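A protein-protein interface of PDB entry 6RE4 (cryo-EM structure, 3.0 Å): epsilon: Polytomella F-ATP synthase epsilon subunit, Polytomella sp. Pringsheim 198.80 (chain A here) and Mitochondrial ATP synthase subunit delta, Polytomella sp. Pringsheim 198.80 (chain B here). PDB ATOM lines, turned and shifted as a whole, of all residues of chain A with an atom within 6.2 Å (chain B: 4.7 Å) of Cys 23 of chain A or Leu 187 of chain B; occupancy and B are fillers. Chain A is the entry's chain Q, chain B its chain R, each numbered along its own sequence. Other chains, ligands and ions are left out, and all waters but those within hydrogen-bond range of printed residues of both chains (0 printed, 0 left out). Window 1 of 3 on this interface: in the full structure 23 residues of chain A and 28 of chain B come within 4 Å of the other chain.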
ATOM      1  N   ARG A  18     -22.103  10.647  -2.726  1.00  0.00           N
ATOM      2  CA  ARG A  18     -22.503  11.586  -1.688  1.00  0.00           C
ATOM      3  C   ARG A  18     -21.860  12.947  -1.877  1.00  0.00           C
ATOM      4  O   ARG A  18     -22.525  13.963  -1.679  1.00  0.00           O
ATOM      5  CB  ARG A  18     -22.161  11.044  -0.314  1.00  0.00           C
ATOM      6  CG  ARG A  18     -22.814  11.835   0.778  1.00  0.00           C
ATOM      7  CD  ARG A  18     -22.632  11.150   2.088  1.00  0.00           C
ATOM      8  NE  ARG A  18     -23.258   9.839   2.092  1.00  0.00           N
ATOM      9  CZ  ARG A  18     -24.331   9.544   2.805  1.00  0.00           C
ATOM     10  NH1 ARG A  18     -24.895  10.469   3.563  1.00  0.00           N
ATOM     11  NH2 ARG A  18     -24.834   8.323   2.759  1.00  0.00           N
ATOM     12  N   TYR A  19     -20.599  12.987  -2.303  1.00  0.00           N
ATOM     13  CA  TYR A  19     -19.914  14.260  -2.492  1.00  0.00           C
ATOM     14  C   TYR A  19     -20.533  15.053  -3.631  1.00  0.00           C
ATOM     15  O   TYR A  19     -20.813  16.250  -3.495  1.00  0.00           O
ATOM     16  CB  TYR A  19     -18.431  14.011  -2.746  1.00  0.00           C
ATOM     17  CG  TYR A  19     -17.738  15.051  -3.590  1.00  0.00           C
ATOM     18  CD1 TYR A  19     -17.405  14.783  -4.912  1.00  0.00           C
ATOM     19  CD2 TYR A  19     -17.388  16.283  -3.061  1.00  0.00           C
ATOM     20  CE1 TYR A  19     -16.771  15.717  -5.686  1.00  0.00           C
ATOM     21  CE2 TYR A  19     -16.749  17.224  -3.833  1.00  0.00           C
ATOM     22  CZ  TYR A  19     -16.442  16.931  -5.145  1.00  0.00           C
ATOM     23  OH  TYR A  19     -15.801  17.859  -5.926  1.00  0.00           O
ATOM     24  N   SER A  20     -20.787  14.396  -4.756  1.00  0.00           N
ATOM     25  CA  SER A  20     -21.332  15.134  -5.877  1.00  0.00           C
ATOM     26  C   SER A  20     -22.813  15.424  -5.678  1.00  0.00           C
ATOM     27  O   SER A  20     -23.328  16.405  -6.221  1.00  0.00           O
ATOM     28  CB  SER A  20     -21.073  14.379  -7.166  1.00  0.00           C
ATOM     29  OG  SER A  20     -21.353  15.204  -8.277  1.00  0.00           O
ATOM     30  N   ASN A  21     -23.500  14.641  -4.844  1.00  0.00           N
ATOM     31  CA  ASN A  21     -24.860  15.005  -4.483  1.00  0.00           C
ATOM     32  C   ASN A  21     -24.899  16.189  -3.531  1.00  0.00           C
ATOM     33  O   ASN A  21     -25.822  17.003  -3.610  1.00  0.00           O
ATOM     34  CB  ASN A  21     -25.573  13.813  -3.873  1.00  0.00           C
ATOM     35  CG  ASN A  21     -26.117  12.889  -4.910  1.00  0.00           C
ATOM     36  OD1 ASN A  21     -27.094  13.200  -5.574  1.00  0.00           O
ATOM     37  ND2 ASN A  21     -25.481  11.748  -5.069  1.00  0.00           N
ATOM     38  N   ILE A  22     -23.922  16.294  -2.626  1.00  0.00           N
ATOM     39  CA  ILE A  22     -23.778  17.492  -1.802  1.00  0.00           C
ATOM     40  C   ILE A  22     -23.558  18.712  -2.679  1.00  0.00           C
ATOM     41  O   ILE A  22     -24.196  19.753  -2.487  1.00  0.00           O
ATOM     42  CB  ILE A  22     -22.634  17.306  -0.787  1.00  0.00           C
ATOM     43  CG1 ILE A  22     -23.063  16.403   0.355  1.00  0.00           C
ATOM     44  CG2 ILE A  22     -22.152  18.622  -0.239  1.00  0.00           C
ATOM     45  CD1 ILE A  22     -21.917  15.952   1.194  1.00  0.00           C
ATOM     46  N   CYS A  23     -22.696  18.577  -3.689  1.00  0.00           N
ATOM     47  CA  CYS A  23     -22.455  19.671  -4.625  1.00  0.00           C
ATOM     48  C   CYS A  23     -23.718  20.047  -5.394  1.00  0.00           C
ATOM     49  O   CYS A  23     -24.007  21.232  -5.578  1.00  0.00           O
ATOM     50  CB  CYS A  23     -21.333  19.295  -5.588  1.00  0.00           C
ATOM     51  SG  CYS A  23     -19.692  19.338  -4.859  1.00  0.00           S
ATOM     52  N   ALA A  24     -24.505  19.054  -5.820  1.00  0.00           N
ATOM     53  CA  ALA A  24     -25.701  19.349  -6.604  1.00  0.00           C
ATOM     54  C   ALA A  24     -26.805  19.960  -5.744  1.00  0.00           C
ATOM     55  O   ALA A  24     -27.510  20.870  -6.196  1.00  0.00           O
ATOM     56  CB  ALA A  24     -26.197  18.091  -7.305  1.00  0.00           C
ATOM     57  N   ASP A  25     -26.961  19.492  -4.503  1.00  0.00           N
ATOM     58  CA  ASP A  25     -27.936  20.100  -3.597  1.00  0.00           C
ATOM     59  C   ASP A  25     -27.543  21.529  -3.240  1.00  0.00           C
ATOM     60  O   ASP A  25     -28.402  22.417  -3.175  1.00  0.00           O
ATOM     61  CB  ASP A  25     -28.080  19.260  -2.326  1.00  0.00           C
ATOM     62  CG  ASP A  25     -28.648  17.874  -2.593  1.00  0.00           C
ATOM     63  OD1 ASP A  25     -28.309  16.932  -1.844  1.00  0.00           O
ATOM     64  OD2 ASP A  25     -29.429  17.723  -3.554  1.00  0.00           O
ATOM     65  N   LEU A  26     -26.248  21.775  -3.039  1.00  0.00           N
ATOM     66  CA  LEU A  26     -25.769  23.127  -2.796  1.00  0.00           C
ATOM     67  C   LEU A  26     -25.924  24.036  -3.999  1.00  0.00           C
ATOM     68  O   LEU A  26     -26.153  25.232  -3.819  1.00  0.00           O
ATOM     69  CB  LEU A  26     -24.308  23.086  -2.371  1.00  0.00           C
ATOM     70  CG  LEU A  26     -23.933  23.071  -0.895  1.00  0.00           C
ATOM     71  CD1 LEU A  26     -24.544  21.934  -0.123  1.00  0.00           C
ATOM     72  CD2 LEU A  26     -22.462  22.897  -0.887  1.00  0.00           C
ATOM     73  N   LEU A  27     -25.801  23.513  -5.211  1.00  0.00           N
ATOM     74  CA  LEU A  27     -26.057  24.353  -6.368  1.00  0.00           C
ATOM     75  C   LEU A  27     -27.543  24.608  -6.551  1.00  0.00           C
ATOM     76  O   LEU A  27     -27.930  25.673  -7.040  1.00  0.00           O
ATOM     77  CB  LEU A  27     -25.467  23.718  -7.624  1.00  0.00           C
ATOM     78  CG  LEU A  27     -25.541  24.483  -8.942  1.00  0.00           C
ATOM     79  CD1 LEU A  27     -25.103  25.908  -8.750  1.00  0.00           C
ATOM     80  CD2 LEU A  27     -24.664  23.812  -9.957  1.00  0.00           C
ATOM     81  N   ARG A  28     -28.389  23.659  -6.156  1.00  0.00           N
ATOM     82  CA  ARG A  28     -29.824  23.897  -6.245  1.00  0.00           C
ATOM     83  C   ARG A  28     -30.292  24.905  -5.209  1.00  0.00           C
ATOM     84  O   ARG A  28     -31.224  25.669  -5.476  1.00  0.00           O
ATOM     85  CB  ARG A  28     -30.590  22.588  -6.089  1.00  0.00           C
ATOM     86  CG  ARG A  28     -30.528  21.713  -7.314  1.00  0.00           C
ATOM     87  CD  ARG A  28     -31.352  20.475  -7.147  1.00  0.00           C
ATOM     88  NE  ARG A  28     -30.788  19.381  -7.920  1.00  0.00           N
ATOM     89  CZ  ARG A  28     -30.234  18.307  -7.380  1.00  0.00           C
ATOM     90  NH1 ARG A  28     -30.167  18.184  -6.064  1.00  0.00           N
ATOM     91  NH2 ARG A  28     -29.744  17.354  -8.153  1.00  0.00           N
ATOM     92  N   PRO B 113     -16.449  22.127  -9.954  1.00  0.00           N
ATOM     93  CA  PRO B 113     -17.471  23.139 -10.263  1.00  0.00           C
ATOM     94  C   PRO B 113     -16.971  24.245 -11.179  1.00  0.00           C
ATOM     95  O   PRO B 113     -16.077  25.007 -10.825  1.00  0.00           O
ATOM     96  CB  PRO B 113     -17.820  23.689  -8.882  1.00  0.00           C
ATOM     97  CG  PRO B 113     -17.647  22.554  -7.994  1.00  0.00           C
ATOM     98  CD  PRO B 113     -16.562  21.694  -8.546  1.00  0.00           C
ATOM     99  N   PHE B 128     -23.234  26.532 -16.118  1.00  0.00           N
ATOM    100  CA  PHE B 128     -22.473  26.234 -14.920  1.00  0.00           C
ATOM    101  C   PHE B 128     -22.930  24.887 -14.391  1.00  0.00           C
ATOM    102  O   PHE B 128     -24.124  24.670 -14.182  1.00  0.00           O
ATOM    103  CB  PHE B 128     -22.656  27.305 -13.853  1.00  0.00           C
ATOM    104  CG  PHE B 128     -21.831  27.077 -12.627  1.00  0.00           C
ATOM    105  CD1 PHE B 128     -20.485  27.375 -12.623  1.00  0.00           C
ATOM    106  CD2 PHE B 128     -22.403  26.583 -11.475  1.00  0.00           C
ATOM    107  CE1 PHE B 128     -19.725  27.182 -11.499  1.00  0.00           C
ATOM    108  CE2 PHE B 128     -21.647  26.384 -10.343  1.00  0.00           C
ATOM    109  CZ  PHE B 128     -20.305  26.684 -10.357  1.00  0.00           C
ATOM    110  N   SER B 130     -22.174  21.324 -11.745  1.00  0.00           N
ATOM    111  CA  SER B 130     -21.886  21.055 -10.351  1.00  0.00           C
ATOM    112  C   SER B 130     -20.648  20.212 -10.143  1.00  0.00           C
ATOM    113  O   SER B 130     -20.163  20.119  -9.013  1.00  0.00           O
ATOM    114  CB  SER B 130     -23.066  20.344  -9.704  1.00  0.00           C
ATOM    115  OG  SER B 130     -22.918  20.355  -8.308  1.00  0.00           O
ATOM    116  N   ALA B 183     -15.885  21.330  -0.136  1.00  0.00           N
ATOM    117  CA  ALA B 183     -16.641  21.255  -1.383  1.00  0.00           C
ATOM    118  C   ALA B 183     -17.564  22.451  -1.549  1.00  0.00           C
ATOM    119  O   ALA B 183     -17.716  22.967  -2.664  1.00  0.00           O
ATOM    120  CB  ALA B 183     -17.445  19.960  -1.427  1.00  0.00           C
ATOM    121  N   ALA B 184     -18.143  22.918  -0.440  1.00  0.00           N
ATOM    122  CA  ALA B 184     -18.996  24.097  -0.449  1.00  0.00           C
ATOM    123  C   ALA B 184     -18.229  25.332  -0.887  1.00  0.00           C
ATOM    124  O   ALA B 184     -18.692  26.087  -1.746  1.00  0.00           O
ATOM    125  CB  ALA B 184     -19.595  24.309   0.939  1.00  0.00           C
ATOM    126  N   ILE B 185     -17.038  25.538  -0.326  1.00  0.00           N
ATOM    127  CA  ILE B 185     -16.327  26.763  -0.656  1.00  0.00           C
ATOM    128  C   ILE B 185     -15.716  26.675  -2.047  1.00  0.00           C
ATOM    129  O   ILE B 185     -15.689  27.677  -2.767  1.00  0.00           O
ATOM    130  CB  ILE B 185     -15.296  27.123   0.438  1.00  0.00           C
ATOM    131  CG1 ILE B 185     -14.764  28.539   0.215  1.00  0.00           C
ATOM    132  CG2 ILE B 185     -14.149  26.124   0.532  1.00  0.00           C
ATOM    133  CD1 ILE B 185     -15.808  29.619   0.334  1.00  0.00           C
ATOM    134  N   GLU B 186     -15.313  25.481  -2.501  1.00  0.00           N
ATOM    135  CA  GLU B 186     -14.748  25.411  -3.845  1.00  0.00           C
ATOM    136  C   GLU B 186     -15.833  25.500  -4.912  1.00  0.00           C
ATOM    137  O   GLU B 186     -15.542  25.875  -6.051  1.00  0.00           O
ATOM    138  CB  GLU B 186     -13.918  24.142  -4.030  1.00  0.00           C
ATOM    139  CG  GLU B 186     -14.715  22.859  -4.140  1.00  0.00           C
ATOM    140  CD  GLU B 186     -13.847  21.631  -4.346  1.00  0.00           C
ATOM    141  OE1 GLU B 186     -12.606  21.768  -4.371  1.00  0.00           O
ATOM    142  OE2 GLU B 186     -14.411  20.528  -4.488  1.00  0.00           O
ATOM    143  N   LEU B 187     -17.085  25.172  -4.570  1.00  0.00           N
ATOM    144  CA  LEU B 187     -18.174  25.386  -5.512  1.00  0.00           C
ATOM    145  C   LEU B 187     -18.634  26.838  -5.506  1.00  0.00           C
ATOM    146  O   LEU B 187     -18.841  27.438  -6.567  1.00  0.00           O
ATOM    147  CB  LEU B 187     -19.336  24.452  -5.183  1.00  0.00           C
ATOM    148  CG  LEU B 187     -20.746  24.825  -5.645  1.00  0.00           C
ATOM    149  CD1 LEU B 187     -20.927  24.724  -7.147  1.00  0.00           C
ATOM    150  CD2 LEU B 187     -21.737  23.940  -4.944  1.00  0.00           C
ATOM    151  N   TYR B 188     -18.779  27.424  -4.319  1.00  0.00           N
ATOM    152  CA  TYR B 188     -19.323  28.771  -4.228  1.00  0.00           C
ATOM    153  C   TYR B 188     -18.320  29.806  -4.699  1.00  0.00           C
ATOM    154  O   TYR B 188     -18.705  30.825  -5.284  1.00  0.00           O
ATOM    155  CB  TYR B 188     -19.762  29.052  -2.797  1.00  0.00           C
ATOM    156  CG  TYR B 188     -21.073  28.401  -2.453  1.00  0.00           C
ATOM    157  CD1 TYR B 188     -22.119  28.409  -3.361  1.00  0.00           C
ATOM    158  CD2 TYR B 188     -21.265  27.773  -1.230  1.00  0.00           C
ATOM    159  CE1 TYR B 188     -23.311  27.815  -3.063  1.00  0.00           C
ATOM    160  CE2 TYR B 188     -22.453  27.168  -0.926  1.00  0.00           C
ATOM    161  CZ  TYR B 188     -23.478  27.198  -1.845  1.00  0.00           C
ATOM    162  OH  TYR B 188     -24.678  26.602  -1.548  1.00  0.00           O
ATOM    163  N   SER B 189     -17.030  29.551  -4.480  1.00  0.00           N
ATOM    164  CA  SER B 189     -16.002  30.474  -4.930  1.00  0.00           C
ATOM    165  C   SER B 189     -15.888  30.470  -6.445  1.00  0.00           C
ATOM    166  O   SER B 189     -15.663  31.520  -7.055  1.00  0.00           O
ATOM    167  CB  SER B 189     -14.674  30.099  -4.285  1.00  0.00           C
ATOM    168  OG  SER B 189     -14.778  30.172  -2.877  1.00  0.00           O
ATOM    169  N   ALA B 190     -16.057  29.304  -7.070  1.00  0.00           N
ATOM    170  CA  ALA B 190     -16.059  29.245  -8.523  1.00  0.00           C
ATOM    171  C   ALA B 190     -17.327  29.849  -9.097  1.00  0.00           C
ATOM    172  O   ALA B 190     -17.296  30.434 -10.185  1.00  0.00           O
ATOM    173  CB  ALA B 190     -15.905  27.804  -8.988  1.00  0.00           C
ATOM    174  N   LEU B 191     -18.445  29.733  -8.378  1.00  0.00           N
ATOM    175  CA  LEU B 191     -19.674  30.392  -8.806  1.00  0.00           C
ATOM    176  C   LEU B 191     -19.616  31.903  -8.606  1.00  0.00           C
ATOM    177  O   LEU B 191     -20.381  32.633  -9.245  1.00  0.00           O
ATOM    178  CB  LEU B 191     -20.864  29.774  -8.064  1.00  0.00           C
ATOM    179  CG  LEU B 191     -22.295  30.150  -8.446  1.00  0.00           C
ATOM    180  CD1 LEU B 191     -22.514  29.891  -9.915  1.00  0.00           C
ATOM    181  CD2 LEU B 191     -23.281  29.346  -7.627  1.00  0.00           C
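O of Tyr 19 of chain A lies within hydrogen-bond range of SG of Cys 23 of chain A.
Cys 23 of chain A touches just these residues of chain B: Ser 130 and Leu 187. Of chain A, only Cys 23 (3.6 Å) and Leu 26 (3.7 Å) come within 4 Å of Leu 187 of chain B. Printed residues of chain A within 4 Å of Ala 183 of chain B: Tyr 19 (3.7 Å). Of the printed residues of chain A, Ala 184 of chain B touches Leu 26 (3.7 Å). Of the printed residues of chain B, Leu 26 of chain A touches Ala 184, Leu 187 and Tyr 188. Of the printed residues of chain B, Tyr 19 of chain A touches Ala 183 (3.7 Å) and Glu 186 (3.3 Å). Ala 190 of chain B touches none of the printed residues of chain A. Ser 20 of chain A touches none of the printed residues of chain B. The nearest residue of chain A that does not touch Leu 187 of chain B is Leu 27 of chain A (4.1 Å).
Hydrophobic or aromatic side chains of chain A within 4 Å of the printed part of chain B: Tyr 19, Leu 26 and Leu 27. Among the printed residues, no Asp or Glu carboxylate lies within 4 Å of a Lys or Arg side-chain nitrogen of the other chain.
Ala 183 of chain B touches Tyr 19 of chain A (CB to CE2, 3.7 Å). Leu 187 of chain B touches Cys 23 of chain A. Ala 184 of chain B touches Leu 26 of chain A (CB to CD2, 3.7 Å). CB of Leu 26 of chain A touches CD2 of Leu 187 of chain B (3.7 Å). CE2 of Phe 128 of chain B touches CD1 of Leu 27 of chain A, at 3.8 Å. Leu 27 of chain A touches Ser 130 of chain B (CD2 to CB, 3.8 Å).
The side-chain hydroxyl of Tyr 19 of chain A lies within hydrogen-bond range of the side-chain carboxylate of Glu 186 of chain B, at 3.3 Å. OG of Ser 130 of chain B is in hydrogen-bond range of N of Ala 24 of chain A. The backbone carbonyl oxygen (O) of Leu 26 of chain A sits at hydrogen-bond distance from the side-chain hydroxyl (OH) of Tyr 188 of chain B (3.0 Å). OG of Ser 130 of chain B sits close to O of Cys 23 of chain A (3.1 Å).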
